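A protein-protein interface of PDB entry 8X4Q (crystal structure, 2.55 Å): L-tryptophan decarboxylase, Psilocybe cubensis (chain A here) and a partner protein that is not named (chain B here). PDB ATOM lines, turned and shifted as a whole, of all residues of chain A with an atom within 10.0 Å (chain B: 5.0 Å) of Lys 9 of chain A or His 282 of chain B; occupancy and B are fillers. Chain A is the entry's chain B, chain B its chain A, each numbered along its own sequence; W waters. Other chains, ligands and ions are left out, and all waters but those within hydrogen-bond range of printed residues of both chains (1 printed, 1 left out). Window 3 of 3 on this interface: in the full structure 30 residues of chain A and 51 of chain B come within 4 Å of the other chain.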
ATOM      1  N   GLY A   6       8.276 -17.861 -13.255  1.00  0.00           N
ATOM      2  CA  GLY A   6       9.459 -18.577 -12.807  1.00  0.00           C
ATOM      3  C   GLY A   6       9.116 -20.009 -12.449  1.00  0.00           C
ATOM      4  O   GLY A   6       8.098 -20.264 -11.805  1.00  0.00           O
ATOM      5  N   LEU A   7       9.971 -20.939 -12.869  1.00  0.00           N
ATOM      6  CA  LEU A   7       9.765 -22.357 -12.597  1.00  0.00           C
ATOM      7  C   LEU A   7      10.986 -22.918 -11.876  1.00  0.00           C
ATOM      8  O   LEU A   7      12.121 -22.493 -12.129  1.00  0.00           O
ATOM      9  CB  LEU A   7       9.482 -23.132 -13.912  1.00  0.00           C
ATOM     10  CG  LEU A   7       8.309 -22.613 -14.769  1.00  0.00           C
ATOM     11  CD1 LEU A   7       8.228 -23.364 -16.075  1.00  0.00           C
ATOM     12  CD2 LEU A   7       6.986 -22.695 -14.037  1.00  0.00           C
ATOM     13  N   ARG A   8      10.758 -23.865 -10.972  1.00  0.00           N
ATOM     14  CA  ARG A   8      11.875 -24.466 -10.252  1.00  0.00           C
ATOM     15  C   ARG A   8      12.566 -25.520 -11.114  1.00  0.00           C
ATOM     16  O   ARG A   8      12.012 -26.001 -12.106  1.00  0.00           O
ATOM     17  CB  ARG A   8      11.408 -25.088  -8.936  1.00  0.00           C
ATOM     18  CG  ARG A   8      10.952 -24.076  -7.922  1.00  0.00           C
ATOM     19  CD  ARG A   8       9.955 -24.659  -6.924  1.00  0.00           C
ATOM     20  NE  ARG A   8       9.009 -25.580  -7.541  1.00  0.00           N
ATOM     21  CZ  ARG A   8       9.028 -26.898  -7.383  1.00  0.00           C
ATOM     22  NH1 ARG A   8       9.955 -27.491  -6.652  1.00  0.00           N
ATOM     23  NH2 ARG A   8       8.097 -27.638  -7.978  1.00  0.00           N
ATOM     24  N   LYS A   9      13.806 -25.871 -10.729  1.00  0.00           N
ATOM     25  CA  LYS A   9      14.533 -26.915 -11.457  1.00  0.00           C
ATOM     26  C   LYS A   9      13.841 -28.256 -11.314  1.00  0.00           C
ATOM     27  O   LYS A   9      13.750 -29.019 -12.285  1.00  0.00           O
ATOM     28  CB  LYS A   9      15.978 -27.036 -10.960  1.00  0.00           C
ATOM     29  N   ASP A  10      13.368 -28.559 -10.099  1.00  0.00           N
ATOM     30  CA  ASP A  10      12.612 -29.781  -9.865  1.00  0.00           C
ATOM     31  C   ASP A  10      11.402 -29.848 -10.778  1.00  0.00           C
ATOM     32  O   ASP A  10      11.056 -30.921 -11.290  1.00  0.00           O
ATOM     33  CB  ASP A  10      12.189 -29.853  -8.402  1.00  0.00           C
ATOM     34  CG  ASP A  10      13.332 -30.269  -7.522  1.00  0.00           C
ATOM     35  OD1 ASP A  10      14.236 -30.941  -8.065  1.00  0.00           O
ATOM     36  OD2 ASP A  10      13.357 -29.902  -6.325  1.00  0.00           O
ATOM     37  N   CYS A  11      10.769 -28.704 -11.008  1.00  0.00           N
ATOM     38  CA  CYS A  11       9.628 -28.628 -11.896  1.00  0.00           C
ATOM     39  C   CYS A  11       9.957 -29.208 -13.260  1.00  0.00           C
ATOM     40  O   CYS A  11      10.841 -28.711 -13.962  1.00  0.00           O
ATOM     41  CB  CYS A  11       9.173 -27.190 -12.056  1.00  0.00           C
ATOM     42  SG  CYS A  11       7.644 -27.176 -12.906  1.00  0.00           S
ATOM     43  N   ARG A  12       9.228 -30.253 -13.641  1.00  0.00           N
ATOM     44  CA  ARG A  12       9.415 -30.882 -14.935  1.00  0.00           C
ATOM     45  C   ARG A  12       8.473 -30.323 -15.999  1.00  0.00           C
ATOM     46  O   ARG A  12       8.389 -30.886 -17.103  1.00  0.00           O
ATOM     47  CB  ARG A  12       9.253 -32.408 -14.809  1.00  0.00           C
ATOM     48  N   ALA A  13       7.776 -29.232 -15.707  1.00  0.00           N
ATOM     49  CA  ALA A  13       7.061 -28.511 -16.750  1.00  0.00           C
ATOM     50  C   ALA A  13       8.040 -27.658 -17.535  1.00  0.00           C
ATOM     51  O   ALA A  13       8.926 -27.017 -16.965  1.00  0.00           O
ATOM     52  CB  ALA A  13       5.965 -27.639 -16.157  1.00  0.00           C
ATOM     53  N   GLU A  14       7.878 -27.650 -18.842  1.00  0.00           N
ATOM     54  CA  GLU A  14       8.894 -27.111 -19.723  1.00  0.00           C
ATOM     55  C   GLU A  14       8.293 -26.022 -20.596  1.00  0.00           C
ATOM     56  O   GLU A  14       7.168 -26.158 -21.096  1.00  0.00           O
ATOM     57  CB  GLU A  14       9.495 -28.229 -20.571  1.00  0.00           C
ATOM     58  CG  GLU A  14      10.118 -29.322 -19.709  1.00  0.00           C
ATOM     59  CD  GLU A  14      11.439 -29.858 -20.242  1.00  0.00           C
ATOM     60  OE1 GLU A  14      12.401 -29.065 -20.406  1.00  0.00           O
ATOM     61  OE2 GLU A  14      11.515 -31.086 -20.471  1.00  0.00           O
ATOM     62  N   LEU A  35       3.871 -29.973 -18.566  1.00  0.00           N
ATOM     63  CA  LEU A  35       4.555 -31.215 -18.241  1.00  0.00           C
ATOM     64  C   LEU A  35       4.587 -32.098 -19.478  1.00  0.00           C
ATOM     65  O   LEU A  35       3.588 -32.217 -20.194  1.00  0.00           O
ATOM     66  CB  LEU A  35       3.856 -31.954 -17.099  1.00  0.00           C
ATOM     67  CG  LEU A  35       3.412 -31.220 -15.833  1.00  0.00           C
ATOM     68  CD1 LEU A  35       2.510 -32.097 -14.960  1.00  0.00           C
ATOM     69  CD2 LEU A  35       4.608 -30.760 -15.041  1.00  0.00           C
ATOM     70  N   ASP B 251      18.567 -22.318 -16.376  1.00  0.00           N
ATOM     71  CA  ASP B 251      19.568 -22.428 -15.312  1.00  0.00           C
ATOM     72  C   ASP B 251      19.895 -21.055 -14.712  1.00  0.00           C
ATOM     73  O   ASP B 251      21.031 -20.576 -14.745  1.00  0.00           O
ATOM     74  CB  ASP B 251      20.826 -23.134 -15.831  1.00  0.00           C
ATOM     75  CG  ASP B 251      21.754 -23.550 -14.711  1.00  0.00           C
ATOM     76  OD1 ASP B 251      21.261 -24.081 -13.681  1.00  0.00           O
ATOM     77  OD2 ASP B 251      22.982 -23.332 -14.857  1.00  0.00           O
ATOM     78  N   VAL B 252      18.852 -20.424 -14.163  1.00  0.00           N
ATOM     79  CA  VAL B 252      18.969 -19.057 -13.660  1.00  0.00           C
ATOM     80  C   VAL B 252      19.708 -19.048 -12.321  1.00  0.00           C
ATOM     81  O   VAL B 252      19.785 -20.064 -11.611  1.00  0.00           O
ATOM     82  CB  VAL B 252      17.573 -18.430 -13.535  1.00  0.00           C
ATOM     83  CG1 VAL B 252      16.975 -18.240 -14.920  1.00  0.00           C
ATOM     84  CG2 VAL B 252      16.679 -19.298 -12.654  1.00  0.00           C
ATOM     85  N   LEU B 267      18.363 -13.901  -9.211  1.00  0.00           N
ATOM     86  CA  LEU B 267      17.186 -14.350  -8.477  1.00  0.00           C
ATOM     87  C   LEU B 267      17.063 -13.634  -7.146  1.00  0.00           C
ATOM     88  O   LEU B 267      15.959 -13.242  -6.748  1.00  0.00           O
ATOM     89  CB  LEU B 267      17.224 -15.858  -8.248  1.00  0.00           C
ATOM     90  CG  LEU B 267      16.809 -16.744  -9.426  1.00  0.00           C
ATOM     91  CD1 LEU B 267      17.265 -18.177  -9.209  1.00  0.00           C
ATOM     92  CD2 LEU B 267      15.332 -16.668  -9.715  1.00  0.00           C
ATOM     93  N   GLN B 279      15.019 -22.176  -3.782  1.00  0.00           N
ATOM     94  CA  GLN B 279      14.315 -23.220  -4.513  1.00  0.00           C
ATOM     95  C   GLN B 279      14.254 -22.946  -6.003  1.00  0.00           C
ATOM     96  O   GLN B 279      13.965 -23.860  -6.785  1.00  0.00           O
ATOM     97  CB  GLN B 279      12.880 -23.352  -4.010  1.00  0.00           C
ATOM     98  CG  GLN B 279      12.769 -23.803  -2.602  1.00  0.00           C
ATOM     99  CD  GLN B 279      11.357 -23.877  -2.177  1.00  0.00           C
ATOM    100  OE1 GLN B 279      10.546 -24.555  -2.816  1.00  0.00           O
ATOM    101  NE2 GLN B 279      11.025 -23.176  -1.096  1.00  0.00           N
ATOM    102  N   PHE B 280      14.465 -21.702  -6.403  1.00  0.00           N
ATOM    103  CA  PHE B 280      14.345 -21.310  -7.790  1.00  0.00           C
ATOM    104  C   PHE B 280      15.701 -21.212  -8.465  1.00  0.00           C
ATOM    105  O   PHE B 280      15.760 -21.017  -9.684  1.00  0.00           O
ATOM    106  CB  PHE B 280      13.567 -19.994  -7.875  1.00  0.00           C
ATOM    107  CG  PHE B 280      12.078 -20.186  -7.776  1.00  0.00           C
ATOM    108  CD1 PHE B 280      11.353 -20.668  -8.866  1.00  0.00           C
ATOM    109  CD2 PHE B 280      11.414 -19.950  -6.581  1.00  0.00           C
ATOM    110  CE1 PHE B 280       9.989 -20.874  -8.776  1.00  0.00           C
ATOM    111  CE2 PHE B 280      10.048 -20.147  -6.483  1.00  0.00           C
ATOM    112  CZ  PHE B 280       9.330 -20.616  -7.579  1.00  0.00           C
ATOM    113  N   GLU B 281      16.780 -21.396  -7.712  1.00  0.00           N
ATOM    114  CA  GLU B 281      18.100 -21.450  -8.312  1.00  0.00           C
ATOM    115  C   GLU B 281      18.161 -22.640  -9.255  1.00  0.00           C
ATOM    116  O   GLU B 281      17.624 -23.707  -8.954  1.00  0.00           O
ATOM    117  CB  GLU B 281      19.182 -21.544  -7.223  1.00  0.00           C
ATOM    118  CG  GLU B 281      19.232 -20.299  -6.303  1.00  0.00           C
ATOM    119  CD  GLU B 281      20.039 -19.111  -6.884  1.00  0.00           C
ATOM    120  OE1 GLU B 281      20.636 -19.248  -7.977  1.00  0.00           O
ATOM    121  OE2 GLU B 281      20.061 -18.025  -6.255  1.00  0.00           O
ATOM    122  N   HIS B 282      18.780 -22.444 -10.419  1.00  0.00           N
ATOM    123  CA  HIS B 282      18.899 -23.450 -11.474  1.00  0.00           C
ATOM    124  C   HIS B 282      17.606 -23.634 -12.264  1.00  0.00           C
ATOM    125  O   HIS B 282      17.511 -24.564 -13.075  1.00  0.00           O
ATOM    126  CB  HIS B 282      19.359 -24.809 -10.923  1.00  0.00           C
ATOM    127  CG  HIS B 282      20.789 -24.818 -10.485  1.00  0.00           C
ATOM    128  ND1 HIS B 282      21.831 -24.557 -11.351  1.00  0.00           N
ATOM    129  CD2 HIS B 282      21.349 -25.031  -9.271  1.00  0.00           C
ATOM    130  CE1 HIS B 282      22.974 -24.615 -10.691  1.00  0.00           C
ATOM    131  NE2 HIS B 282      22.710 -24.904  -9.429  1.00  0.00           N
ATOM    132  N   GLY B 283      16.617 -22.766 -12.069  1.00  0.00           N
ATOM    133  CA  GLY B 283      15.342 -22.872 -12.737  1.00  0.00           C
ATOM    134  C   GLY B 283      15.308 -22.137 -14.062  1.00  0.00           C
ATOM    135  O   GLY B 283      16.341 -21.856 -14.685  1.00  0.00           O
ATOM    136  N   SER B 284      14.088 -21.811 -14.497  1.00  0.00           N
ATOM    137  CA  SER B 284      13.896 -21.085 -15.744  1.00  0.00           C
ATOM    138  C   SER B 284      12.873 -19.970 -15.566  1.00  0.00           C
ATOM    139  O   SER B 284      11.961 -20.058 -14.737  1.00  0.00           O
ATOM    140  CB  SER B 284      13.457 -22.026 -16.877  1.00  0.00           C
ATOM    141  OG  SER B 284      12.358 -22.800 -16.448  1.00  0.00           O
HETATM  142  O   HOH W   1      11.554 -26.604  -4.615  1.00  0.00           O
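Water W1 lies within hydrogen-bond range of NH1 of Arg 8 of chain A (2.7 Å) and OE1 of Gln 279 of chain B (2.9 Å).
O of Ser 284 of chain B is in hydrogen-bond range of N of Leu 7 of chain A (2.9 Å).
Lys 9 of chain A touches just these residues of chain B: His 282 and Gly 283. Of chain A, only Lys 9 comes within 4 Å of His 282 of chain B. Asp 251 of chain B touches none of the printed residues of chain A. Gly 283 of chain B touches just these residues of chain A: Leu 7 (3.3 Å) and Lys 9 (3.9 Å). Printed residues of chain A within 4 Å of Phe 280 of chain B: Gly 6 (3.6 Å), Leu 7 (3.8 Å) and Arg 8 (3.5 Å). Of the printed residues of chain B, Gly 6 of chain A touches Phe 280 (3.6 Å) and Ser 284 (3.5 Å).
The side-chain carboxylate of Asp 251 of chain B sits at hydrogen-bond distance from a ring nitrogen (ND1) of His 282 of chain B (2.4 Å). The backbone NH of Asp 251 of chain B sits at hydrogen-bond distance from the backbone carbonyl oxygen of Gly 283 of chain B (2.8 Å). N of His 282 of chain B sits at hydrogen-bond distance from O of Val 252 of chain B. The backbone NH (N) of Val 252 of chain B is in hydrogen-bond range of the backbone carbonyl oxygen (O) of Gly 283 of chain B (2.9 Å).
Gly 6 of chain A touches Phe 280 of chain B (O to CE1, 3.6 Å). Gly 6 of chain A touches Ser 284 of chain B (CA to O, 3.5 Å). Phe 280 of chain B touches Leu 7 of chain A (CD1 to C, 3.8 Å). CA of Gly 283 of chain B touches O of Leu 7 of chain A, 3.3 Å away. Arg 8 of chain A touches Gln 279 of chain B. Phe 280 of chain B touches Arg 8 of chain A. O of His 282 of chain B touches CB of Lys 9 of chain A (3.6 Å). Gly 283 of chain B touches Lys 9 of chain A.
Printed residues of chain A that touch a printed residue of chain B: Gly 6, Leu 7, Arg 8 and Lys 9. Hydrophobic or aromatic side chains of chain A within 4 Å of the printed part of chain B: Leu 7. Printed residues of chain B that touch a printed residue of chain A: Gln 279, Phe 280, His 282, Gly 283 and Ser 284. Among the printed residues, 9 pairs touch across the chains. Among the printed residues, no Asp or Glu carboxylate lies within 4 Å of a Lys or Arg side-chain nitrogen of the other chain.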
